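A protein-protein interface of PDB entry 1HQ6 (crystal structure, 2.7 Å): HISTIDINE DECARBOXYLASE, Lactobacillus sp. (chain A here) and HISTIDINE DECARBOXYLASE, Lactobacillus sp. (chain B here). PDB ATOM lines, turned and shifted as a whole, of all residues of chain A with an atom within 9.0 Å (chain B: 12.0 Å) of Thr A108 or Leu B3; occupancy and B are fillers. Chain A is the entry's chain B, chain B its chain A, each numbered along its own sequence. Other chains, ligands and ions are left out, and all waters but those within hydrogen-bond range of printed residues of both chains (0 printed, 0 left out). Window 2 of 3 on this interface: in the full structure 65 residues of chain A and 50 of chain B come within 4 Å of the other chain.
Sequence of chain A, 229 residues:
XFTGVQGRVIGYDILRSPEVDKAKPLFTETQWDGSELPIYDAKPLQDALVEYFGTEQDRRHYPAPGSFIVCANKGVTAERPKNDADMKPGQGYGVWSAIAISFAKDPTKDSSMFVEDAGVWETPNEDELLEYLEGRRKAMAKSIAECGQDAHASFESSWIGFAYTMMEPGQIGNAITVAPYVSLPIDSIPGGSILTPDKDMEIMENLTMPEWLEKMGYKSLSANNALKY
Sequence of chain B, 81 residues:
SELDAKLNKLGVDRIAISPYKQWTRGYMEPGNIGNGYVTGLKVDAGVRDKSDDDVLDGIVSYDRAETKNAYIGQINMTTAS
OH of Tyr B37 lies within hydrogen-bond range of N of Gly A4, at 2.7 Å. The backbone carbonyl oxygen (O) of Arg B14 sits at hydrogen-bond distance from the guanidinium group (NH1) of Arg A8, 3.2 Å away. The backbone carbonyl oxygen (O) of Gln A6 lies within hydrogen-bond range of the backbone NH (N) of Tyr B37, at 2.9 Å. NH2 of Arg B14 lies within salt-bridge range of OE2 of Glu A205, at 3.8 Å. N of Arg A8 is in hydrogen-bond range of O of Tyr B37 (3.3 Å). The side-chain hydroxyl (OG) of Ser B1 sits at hydrogen-bond distance from the side-chain carboxylate (OE1) of Glu A205, at 2.8 Å. The guanidinium group (NE) of Arg B14 sits at hydrogen-bond distance from the backbone carbonyl oxygen (O) of Gly A7 (3.2 Å). The side-chain carboxylate (OE2) of Glu A205 sits close to the side-chain carboxylate (OD2) of Asp B4 (3.4 Å). The side-chain carboxylate (OD2) of Asp B4 lies within salt-bridge range of the guanidinium group (NH2) of Arg A8 (2.8 Å).
Thr A108 touches just one residue of chain B: Leu B3. Of chain A, only Thr A108 (3.7 Å) comes within 4 Å of Leu B3. Val A5 touches just these residues of chain B: Leu B7 (3.2 Å), Val B12 (3.4 Å) and Arg B14 (3.5 Å). No residue of chain B comes within 4 Å of Asp A106. No residue of chain B comes within 4 Å of Pro A107. No residue of chain B comes within 4 Å of Lys A109. No residue of chain B comes within 4 Å of Asp A110. Of chain A, only Arg A8 and Glu A205 come within 4 Å of Asp B4. Printed residues of chain B within 4 Å of Glu A205: Ser B1 (2.8 Å), Asp B4 (3.4 Å) and Arg B14 (3.8 Å). Printed residues of chain A within 4 Å of Arg B14: Val A5, Gln A6, Gly A7, Arg A8 and Glu A205. Lys B6 touches none of the printed residues of chain A.
Printed residues of chain A that touch a printed residue of chain B: Gly A4, Val A5, Gln A6, Gly A7, Arg A8, Thr A108 and Glu A205. Of the 16 printed residues of chain B, 7 touch a printed residue of chain A. Printed residues of chain B that touch a printed residue of chain A: Ser B1, Leu B3, Asp B4, Leu B7, Val B12, Arg B14 and Tyr B37. Hydrophobic or aromatic side chains of chain B that line the printed part of chain A: Leu B3, Leu B7, Val B12 and Tyr B37.
The side-chain carboxylate (OD2) of Asp B4 is in salt-bridge range of the guanidinium group (NH2) of Arg B14 (3.1 Å). The backbone carbonyl oxygen (O) of Leu B7 sits at hydrogen-bond distance from the backbone NH (N) of Val B12, at 3.2 Å. The side-chain carboxylate of Asp A106 lies within hydrogen-bond range of the side-chain hydroxyl of Thr A108, at 2.7 Å. The side-chain carboxylate of Asp B4 sits at hydrogen-bond distance from the side-chain hydroxyl of Ser B1. O of Val B12 sits at hydrogen-bond distance from ND2 of Asn B8, 2.9 Å away. The guanidinium group (NH2) of Arg A8 lies within salt-bridge range of the side-chain carboxylate (OE2) of Glu A205.
Leu B7 touches Val A5 (CD2 to O, 3.2 Å). Val B12 touches Val A5 (CG1 to O, 3.4 Å). Arg B14 touches Val A5. Gln A6 touches Arg B14 (C to CG, 3.6 Å). Tyr B37 touches Gly A7 (O to CA, 3.1 Å). CD1 of Leu B3 touches CG2 of Thr A108, at 3.7 Å.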
ATOM      1  N   GLY A   4     -16.195  22.686   9.678  1.00  0.00           N
ATOM      2  CA  GLY A   4     -15.496  23.635  10.521  1.00  0.00           C
ATOM      3  C   GLY A   4     -14.155  24.039   9.983  1.00  0.00           C
ATOM      4  O   GLY A   4     -13.966  24.358   8.805  1.00  0.00           O
ATOM      5  N   VAL A   5     -13.189  23.948  10.877  1.00  0.00           N
ATOM      6  CA  VAL A   5     -11.838  24.352  10.518  1.00  0.00           C
ATOM      7  C   VAL A   5     -11.240  23.596   9.332  1.00  0.00           C
ATOM      8  O   VAL A   5     -10.390  24.141   8.657  1.00  0.00           O
ATOM      9  CB  VAL A   5     -10.899  24.216  11.739  1.00  0.00           C
ATOM     10  CG1 VAL A   5     -11.374  25.212  12.764  1.00  0.00           C
ATOM     11  CG2 VAL A   5     -10.897  22.831  12.337  1.00  0.00           C
ATOM     12  N   GLN A   6     -11.673  22.393   8.967  1.00  0.00           N
ATOM     13  CA  GLN A   6     -11.043  21.663   7.886  1.00  0.00           C
ATOM     14  C   GLN A   6     -11.823  21.749   6.593  1.00  0.00           C
ATOM     15  O   GLN A   6     -11.528  20.993   5.661  1.00  0.00           O
ATOM     16  CB  GLN A   6     -10.922  20.202   8.238  1.00  0.00           C
ATOM     17  CG  GLN A   6     -10.160  19.872   9.477  1.00  0.00           C
ATOM     18  CD  GLN A   6     -10.799  18.680  10.132  1.00  0.00           C
ATOM     19  OE1 GLN A   6     -10.402  17.520  10.018  1.00  0.00           O
ATOM     20  NE2 GLN A   6     -11.873  18.943  10.856  1.00  0.00           N
ATOM     21  N   GLY A   7     -12.806  22.615   6.442  1.00  0.00           N
ATOM     22  CA  GLY A   7     -13.656  22.430   5.296  1.00  0.00           C
ATOM     23  C   GLY A   7     -13.965  23.634   4.477  1.00  0.00           C
ATOM     24  O   GLY A   7     -13.811  24.784   4.879  1.00  0.00           O
ATOM     25  N   ARG A   8     -14.443  23.286   3.299  1.00  0.00           N
ATOM     26  CA  ARG A   8     -14.865  24.234   2.308  1.00  0.00           C
ATOM     27  C   ARG A   8     -16.201  23.778   1.759  1.00  0.00           C
ATOM     28  O   ARG A   8     -16.501  22.583   1.801  1.00  0.00           O
ATOM     29  CB  ARG A   8     -13.843  24.297   1.193  1.00  0.00           C
ATOM     30  CG  ARG A   8     -12.664  25.155   1.585  1.00  0.00           C
ATOM     31  CD  ARG A   8     -11.726  25.394   0.413  1.00  0.00           C
ATOM     32  NE  ARG A   8     -10.539  26.145   0.806  1.00  0.00           N
ATOM     33  CZ  ARG A   8      -9.378  25.550   1.068  1.00  0.00           C
ATOM     34  NH1 ARG A   8      -9.217  24.229   0.976  1.00  0.00           N
ATOM     35  NH2 ARG A   8      -8.370  26.300   1.472  1.00  0.00           N
ATOM     36  N   TYR A  12     -19.444  28.072  -2.509  1.00  0.00           N
ATOM     37  CA  TYR A  12     -19.306  29.278  -1.694  1.00  0.00           C
ATOM     38  C   TYR A  12     -17.834  29.515  -1.488  1.00  0.00           C
ATOM     39  O   TYR A  12     -17.352  30.592  -1.811  1.00  0.00           O
ATOM     40  CB  TYR A  12     -19.982  29.129  -0.334  1.00  0.00           C
ATOM     41  CG  TYR A  12     -19.942  30.349   0.592  1.00  0.00           C
ATOM     42  CD1 TYR A  12     -20.923  31.342   0.514  1.00  0.00           C
ATOM     43  CD2 TYR A  12     -18.962  30.447   1.575  1.00  0.00           C
ATOM     44  CE1 TYR A  12     -20.930  32.412   1.413  1.00  0.00           C
ATOM     45  CE2 TYR A  12     -18.964  31.511   2.472  1.00  0.00           C
ATOM     46  CZ  TYR A  12     -19.949  32.480   2.391  1.00  0.00           C
ATOM     47  OH  TYR A  12     -19.973  33.506   3.309  1.00  0.00           O
ATOM     48  N   ASP A  13     -17.123  28.525  -0.947  1.00  0.00           N
ATOM     49  CA  ASP A  13     -15.695  28.637  -0.695  1.00  0.00           C
ATOM     50  C   ASP A  13     -14.898  28.253  -1.912  1.00  0.00           C
ATOM     51  O   ASP A  13     -13.769  28.686  -2.082  1.00  0.00           O
ATOM     52  CB  ASP A  13     -15.262  27.728   0.406  1.00  0.00           C
ATOM     53  CG  ASP A  13     -15.911  28.048   1.741  1.00  0.00           C
ATOM     54  OD1 ASP A  13     -16.721  27.249   2.227  1.00  0.00           O
ATOM     55  OD2 ASP A  13     -15.605  29.102   2.294  1.00  0.00           O
ATOM     56  N   ALA A 104     -19.965  30.448   9.712  1.00  0.00           N
ATOM     57  CA  ALA A 104     -19.565  31.075  10.957  1.00  0.00           C
ATOM     58  C   ALA A 104     -18.790  32.350  10.713  1.00  0.00           C
ATOM     59  O   ALA A 104     -18.054  32.474   9.733  1.00  0.00           O
ATOM     60  CB  ALA A 104     -18.692  30.156  11.760  1.00  0.00           C
ATOM     61  N   LYS A 105     -18.952  33.319  11.607  1.00  0.00           N
ATOM     62  CA  LYS A 105     -18.297  34.613  11.493  1.00  0.00           C
ATOM     63  C   LYS A 105     -16.793  34.358  11.594  1.00  0.00           C
ATOM     64  O   LYS A 105     -16.016  34.798  10.749  1.00  0.00           O
ATOM     65  CB  LYS A 105     -18.766  35.527  12.641  1.00  0.00           C
ATOM     66  CG  LYS A 105     -18.842  37.041  12.397  1.00  0.00           C
ATOM     67  CD  LYS A 105     -20.168  37.480  11.784  1.00  0.00           C
ATOM     68  CE  LYS A 105     -21.013  38.263  12.809  1.00  0.00           C
ATOM     69  NZ  LYS A 105     -22.207  38.792  12.161  1.00  0.00           N
ATOM     70  N   ASP A 106     -16.343  33.612  12.608  1.00  0.00           N
ATOM     71  CA  ASP A 106     -14.927  33.348  12.746  1.00  0.00           C
ATOM     72  C   ASP A 106     -14.627  31.865  12.630  1.00  0.00           C
ATOM     73  O   ASP A 106     -14.577  31.173  13.655  1.00  0.00           O
ATOM     74  CB  ASP A 106     -14.440  33.866  14.100  1.00  0.00           C
ATOM     75  CG  ASP A 106     -12.925  33.814  14.288  1.00  0.00           C
ATOM     76  OD1 ASP A 106     -12.193  33.650  13.301  1.00  0.00           O
ATOM     77  OD2 ASP A 106     -12.482  33.952  15.433  1.00  0.00           O
ATOM     78  N   PRO A 107     -14.322  31.311  11.455  1.00  0.00           N
ATOM     79  CA  PRO A 107     -14.089  29.886  11.258  1.00  0.00           C
ATOM     80  C   PRO A 107     -12.798  29.375  11.887  1.00  0.00           C
ATOM     81  O   PRO A 107     -12.393  28.243  11.668  1.00  0.00           O
ATOM     82  CB  PRO A 107     -14.115  29.724   9.770  1.00  0.00           C
ATOM     83  CG  PRO A 107     -14.602  31.037   9.195  1.00  0.00           C
ATOM     84  CD  PRO A 107     -14.109  32.037  10.217  1.00  0.00           C
ATOM     85  N   THR A 108     -12.058  30.192  12.622  1.00  0.00           N
ATOM     86  CA  THR A 108     -10.877  29.713  13.302  1.00  0.00           C
ATOM     87  C   THR A 108     -11.243  29.332  14.734  1.00  0.00           C
ATOM     88  O   THR A 108     -10.451  28.736  15.475  1.00  0.00           O
ATOM     89  CB  THR A 108      -9.847  30.807  13.331  1.00  0.00           C
ATOM     90  OG1 THR A 108     -10.409  31.779  14.198  1.00  0.00           O
ATOM     91  CG2 THR A 108      -9.581  31.464  11.995  1.00  0.00           C
ATOM     92  N   LYS A 109     -12.410  29.805  15.163  1.00  0.00           N
ATOM     93  CA  LYS A 109     -12.832  29.592  16.528  1.00  0.00           C
ATOM     94  C   LYS A 109     -14.114  28.804  16.573  1.00  0.00           C
ATOM     95  O   LYS A 109     -14.259  27.932  17.425  1.00  0.00           O
ATOM     96  CB  LYS A 109     -13.039  30.928  17.206  1.00  0.00           C
ATOM     97  CG  LYS A 109     -12.645  30.931  18.673  1.00  0.00           C
ATOM     98  CD  LYS A 109     -13.074  32.215  19.397  1.00  0.00           C
ATOM     99  CE  LYS A 109     -12.578  32.258  20.865  1.00  0.00           C
ATOM    100  NZ  LYS A 109     -13.043  31.130  21.674  1.00  0.00           N
ATOM    101  N   ASP A 110     -15.055  29.082  15.682  1.00  0.00           N
ATOM    102  CA  ASP A 110     -16.342  28.417  15.716  1.00  0.00           C
ATOM    103  C   ASP A 110     -16.535  27.692  14.408  1.00  0.00           C
ATOM    104  O   ASP A 110     -15.915  28.060  13.400  1.00  0.00           O
ATOM    105  CB  ASP A 110     -17.508  29.387  15.843  1.00  0.00           C
ATOM    106  CG  ASP A 110     -17.618  30.172  17.137  1.00  0.00           C
ATOM    107  OD1 ASP A 110     -17.507  29.579  18.219  1.00  0.00           O
ATOM    108  OD2 ASP A 110     -17.826  31.384  17.044  1.00  0.00           O
ATOM    109  N   SER A 111     -17.442  26.711  14.402  1.00  0.00           N
ATOM    110  CA  SER A 111     -17.764  25.960  13.201  1.00  0.00           C
ATOM    111  C   SER A 111     -18.993  26.492  12.527  1.00  0.00           C
ATOM    112  O   SER A 111     -19.782  27.246  13.100  1.00  0.00           O
ATOM    113  CB  SER A 111     -17.998  24.518  13.545  1.00  0.00           C
ATOM    114  OG  SER A 111     -18.314  23.679  12.441  1.00  0.00           O
ATOM    115  N   SER A 112     -19.115  26.091  11.277  1.00  0.00           N
ATOM    116  CA  SER A 112     -20.266  26.397  10.480  1.00  0.00           C
ATOM    117  C   SER A 112     -21.176  25.191  10.632  1.00  0.00           C
ATOM    118  O   SER A 112     -20.728  24.048  10.781  1.00  0.00           O
ATOM    119  CB  SER A 112     -19.792  26.615   9.056  1.00  0.00           C
ATOM    120  OG  SER A 112     -18.871  27.716   9.030  1.00  0.00           O
ATOM    121  N   GLU A 205     -10.396  27.337  -5.068  1.00  0.00           N
ATOM    122  CA  GLU A 205     -10.833  28.414  -4.215  1.00  0.00           C
ATOM    123  C   GLU A 205     -10.907  29.711  -5.013  1.00  0.00           C
ATOM    124  O   GLU A 205     -11.582  30.655  -4.630  1.00  0.00           O
ATOM    125  CB  GLU A 205      -9.819  28.423  -3.082  1.00  0.00           C
ATOM    126  CG  GLU A 205      -9.717  29.576  -2.125  1.00  0.00           C
ATOM    127  CD  GLU A 205      -8.702  29.280  -1.029  1.00  0.00           C
ATOM    128  OE1 GLU A 205      -7.532  29.620  -1.203  1.00  0.00           O
ATOM    129  OE2 GLU A 205      -9.065  28.719   0.007  1.00  0.00           O
ATOM    130  N   SER B   1      -5.444  32.441   0.847  1.00  0.00           N
ATOM    131  CA  SER B   1      -6.640  32.942   1.508  1.00  0.00           C
ATOM    132  C   SER B   1      -6.068  33.160   2.880  1.00  0.00           C
ATOM    133  O   SER B   1      -5.407  32.249   3.386  1.00  0.00           O
ATOM    134  CB  SER B   1      -7.710  31.844   1.509  1.00  0.00           C
ATOM    135  OG  SER B   1      -6.986  30.622   1.325  1.00  0.00           O
ATOM    136  N   GLU B   2      -6.235  34.343   3.462  1.00  0.00           N
ATOM    137  CA  GLU B   2      -5.690  34.618   4.780  1.00  0.00           C
ATOM    138  C   GLU B   2      -6.128  33.542   5.763  1.00  0.00           C
ATOM    139  O   GLU B   2      -5.315  33.068   6.539  1.00  0.00           O
ATOM    140  CB  GLU B   2      -6.175  35.995   5.216  1.00  0.00           C
ATOM    141  CG  GLU B   2      -5.131  37.111   5.279  1.00  0.00           C
ATOM    142  CD  GLU B   2      -4.408  37.217   6.638  1.00  0.00           C
ATOM    143  OE1 GLU B   2      -4.807  38.066   7.461  1.00  0.00           O
ATOM    144  OE2 GLU B   2      -3.444  36.460   6.867  1.00  0.00           O
ATOM    145  N   LEU B   3      -7.364  33.043   5.637  1.00  0.00           N
ATOM    146  CA  LEU B   3      -7.915  32.054   6.543  1.00  0.00           C
ATOM    147  C   LEU B   3      -7.005  30.845   6.646  1.00  0.00           C
ATOM    148  O   LEU B   3      -6.587  30.475   7.739  1.00  0.00           O
ATOM    149  CB  LEU B   3      -9.306  31.656   6.047  1.00  0.00           C
ATOM    150  CG  LEU B   3     -10.110  30.705   6.917  1.00  0.00           C
ATOM    151  CD1 LEU B   3     -10.266  31.243   8.318  1.00  0.00           C
ATOM    152  CD2 LEU B   3     -11.446  30.511   6.278  1.00  0.00           C
ATOM    153  N   ASP B   4      -6.624  30.268   5.520  1.00  0.00           N
ATOM    154  CA  ASP B   4      -5.715  29.146   5.521  1.00  0.00           C
ATOM    155  C   ASP B   4      -4.405  29.440   6.216  1.00  0.00           C
ATOM    156  O   ASP B   4      -3.903  28.589   6.945  1.00  0.00           O
ATOM    157  CB  ASP B   4      -5.481  28.749   4.106  1.00  0.00           C
ATOM    158  CG  ASP B   4      -6.676  27.951   3.631  1.00  0.00           C
ATOM    159  OD1 ASP B   4      -6.701  26.756   3.914  1.00  0.00           O
ATOM    160  OD2 ASP B   4      -7.588  28.493   3.006  1.00  0.00           O
ATOM    161  N   ALA B   5      -3.859  30.647   6.089  1.00  0.00           N
ATOM    162  CA  ALA B   5      -2.637  30.974   6.806  1.00  0.00           C
ATOM    163  C   ALA B   5      -2.875  30.915   8.295  1.00  0.00           C
ATOM    164  O   ALA B   5      -2.102  30.281   8.992  1.00  0.00           O
ATOM    165  CB  ALA B   5      -2.165  32.371   6.487  1.00  0.00           C
ATOM    166  N   LYS B   6      -3.964  31.504   8.793  1.00  0.00           N
ATOM    167  CA  LYS B   6      -4.345  31.519  10.205  1.00  0.00           C
ATOM    168  C   LYS B   6      -4.606  30.115  10.723  1.00  0.00           C
ATOM    169  O   LYS B   6      -4.235  29.678  11.818  1.00  0.00           O
ATOM    170  CB  LYS B   6      -5.620  32.327  10.413  1.00  0.00           C
ATOM    171  CG  LYS B   6      -5.512  33.807  10.060  1.00  0.00           C
ATOM    172  CD  LYS B   6      -6.741  34.583  10.505  1.00  0.00           C
ATOM    173  CE  LYS B   6      -6.433  36.076  10.467  1.00  0.00           C
ATOM    174  NZ  LYS B   6      -7.586  36.884  10.828  1.00  0.00           N
ATOM    175  N   LEU B   7      -5.246  29.356   9.867  1.00  0.00           N
ATOM    176  CA  LEU B   7      -5.591  27.988  10.153  1.00  0.00           C
ATOM    177  C   LEU B   7      -4.344  27.134  10.261  1.00  0.00           C
ATOM    178  O   LEU B   7      -4.185  26.385  11.231  1.00  0.00           O
ATOM    179  CB  LEU B   7      -6.481  27.491   9.045  1.00  0.00           C
ATOM    180  CG  LEU B   7      -7.817  26.876   9.346  1.00  0.00           C
ATOM    181  CD1 LEU B   7      -8.657  27.739  10.253  1.00  0.00           C
ATOM    182  CD2 LEU B   7      -8.515  26.690   8.023  1.00  0.00           C
ATOM    183  N   ASN B   8      -3.409  27.271   9.309  1.00  0.00           N
ATOM    184  CA  ASN B   8      -2.198  26.463   9.264  1.00  0.00           C
ATOM    185  C   ASN B   8      -1.347  26.693  10.493  1.00  0.00           C
ATOM    186  O   ASN B   8      -0.744  25.762  11.026  1.00  0.00           O
ATOM    187  CB  ASN B   8      -1.392  26.779   8.021  1.00  0.00           C
ATOM    188  CG  ASN B   8      -1.957  26.235   6.717  1.00  0.00           C
ATOM    189  OD1 ASN B   8      -1.657  26.712   5.628  1.00  0.00           O
ATOM    190  ND2 ASN B   8      -2.769  25.207   6.679  1.00  0.00           N
ATOM    191  N   LYS B   9      -1.354  27.904  11.041  1.00  0.00           N
ATOM    192  CA  LYS B   9      -0.601  28.190  12.258  1.00  0.00           C
ATOM    193  C   LYS B   9      -1.136  27.426  13.474  1.00  0.00           C
ATOM    194  O   LYS B   9      -0.490  27.346  14.519  1.00  0.00           O
ATOM    195  CB  LYS B   9      -0.628  29.706  12.522  1.00  0.00           C
ATOM    196  CG  LYS B   9       0.052  30.456  11.360  1.00  0.00           C
ATOM    197  CD  LYS B   9       0.204  31.984  11.465  1.00  0.00           C
ATOM    198  CE  LYS B   9       1.211  32.415  12.520  1.00  0.00           C
ATOM    199  NZ  LYS B   9       1.443  33.846  12.433  1.00  0.00           N
ATOM    200  N   LEU B  10      -2.343  26.863  13.380  1.00  0.00           N
ATOM    201  CA  LEU B  10      -2.946  26.111  14.459  1.00  0.00           C
ATOM    202  C   LEU B  10      -2.760  24.628  14.213  1.00  0.00           C
ATOM    203  O   LEU B  10      -3.053  23.788  15.061  1.00  0.00           O
ATOM    204  CB  LEU B  10      -4.423  26.447  14.529  1.00  0.00           C
ATOM    205  CG  LEU B  10      -4.873  27.898  14.761  1.00  0.00           C
ATOM    206  CD1 LEU B  10      -6.364  28.035  14.551  1.00  0.00           C
ATOM    207  CD2 LEU B  10      -4.468  28.313  16.167  1.00  0.00           C
ATOM    208  N   GLY B  11      -2.241  24.231  13.079  1.00  0.00           N
ATOM    209  CA  GLY B  11      -2.034  22.832  12.805  1.00  0.00           C
ATOM    210  C   GLY B  11      -3.077  22.355  11.840  1.00  0.00           C
ATOM    211  O   GLY B  11      -3.015  21.239  11.336  1.00  0.00           O
ATOM    212  N   VAL B  12      -4.042  23.197  11.480  1.00  0.00           N
ATOM    213  CA  VAL B  12      -5.149  22.778  10.631  1.00  0.00           C
ATOM    214  C   VAL B  12      -4.853  23.088   9.178  1.00  0.00           C
ATOM    215  O   VAL B  12      -4.310  24.144   8.880  1.00  0.00           O
ATOM    216  CB  VAL B  12      -6.410  23.518  11.024  1.00  0.00           C
ATOM    217  CG1 VAL B  12      -7.569  22.994  10.221  1.00  0.00           C
ATOM    218  CG2 VAL B  12      -6.697  23.344  12.489  1.00  0.00           C
ATOM    219  N   ASP B  13      -5.213  22.225   8.249  1.00  0.00           N
ATOM    220  CA  ASP B  13      -5.103  22.485   6.825  1.00  0.00           C
ATOM    221  C   ASP B  13      -6.412  22.033   6.189  1.00  0.00           C
ATOM    222  O   ASP B  13      -7.004  21.059   6.634  1.00  0.00           O
ATOM    223  CB  ASP B  13      -3.958  21.692   6.193  1.00  0.00           C
ATOM    224  CG  ASP B  13      -4.055  20.166   6.206  1.00  0.00           C
ATOM    225  OD1 ASP B  13      -4.611  19.616   5.258  1.00  0.00           O
ATOM    226  OD2 ASP B  13      -3.560  19.542   7.149  1.00  0.00           O
ATOM    227  N   ARG B  14      -6.883  22.645   5.121  1.00  0.00           N
ATOM    228  CA  ARG B  14      -8.129  22.215   4.518  1.00  0.00           C
ATOM    229  C   ARG B  14      -7.878  21.419   3.256  1.00  0.00           C
ATOM    230  O   ARG B  14      -8.712  21.402   2.360  1.00  0.00           O
ATOM    231  CB  ARG B  14      -8.979  23.435   4.178  1.00  0.00           C
ATOM    232  CG  ARG B  14      -9.585  24.255   5.303  1.00  0.00           C
ATOM    233  CD  ARG B  14      -9.729  25.603   4.679  1.00  0.00           C
ATOM    234  NE  ARG B  14     -10.962  26.262   5.014  1.00  0.00           N
ATOM    235  CZ  ARG B  14     -11.355  27.341   4.335  1.00  0.00           C
ATOM    236  NH1 ARG B  14     -12.503  27.920   4.667  1.00  0.00           N
ATOM    237  NH2 ARG B  14     -10.648  27.863   3.337  1.00  0.00           N
ATOM    238  N   ILE B  15      -6.756  20.724   3.104  1.00  0.00           N
ATOM    239  CA  ILE B  15      -6.443  20.052   1.835  1.00  0.00           C
ATOM    240  C   ILE B  15      -7.184  18.731   1.817  1.00  0.00           C
ATOM    241  O   ILE B  15      -7.204  18.036   2.832  1.00  0.00           O
ATOM    242  CB  ILE B  15      -4.932  19.799   1.713  1.00  0.00           C
ATOM    243  CG1 ILE B  15      -4.177  21.080   1.916  1.00  0.00           C
ATOM    244  CG2 ILE B  15      -4.600  19.276   0.346  1.00  0.00           C
ATOM    245  CD1 ILE B  15      -2.735  20.863   2.390  1.00  0.00           C
ATOM    246  N   TYR B  37     -11.673  18.415   4.327  1.00  0.00           N
ATOM    247  CA  TYR B  37     -12.821  17.854   3.674  1.00  0.00           C
ATOM    248  C   TYR B  37     -13.546  18.928   2.911  1.00  0.00           C
ATOM    249  O   TYR B  37     -13.433  20.117   3.221  1.00  0.00           O
ATOM    250  CB  TYR B  37     -13.717  17.212   4.713  1.00  0.00           C
ATOM    251  CG  TYR B  37     -14.121  18.006   5.933  1.00  0.00           C
ATOM    252  CD1 TYR B  37     -14.956  19.105   5.798  1.00  0.00           C
ATOM    253  CD2 TYR B  37     -13.719  17.597   7.200  1.00  0.00           C
ATOM    254  CE1 TYR B  37     -15.399  19.808   6.913  1.00  0.00           C
ATOM    255  CE2 TYR B  37     -14.167  18.295   8.329  1.00  0.00           C
ATOM    256  CZ  TYR B  37     -15.004  19.399   8.170  1.00  0.00           C
ATOM    257  OH  TYR B  37     -15.486  20.081   9.247  1.00  0.00           O
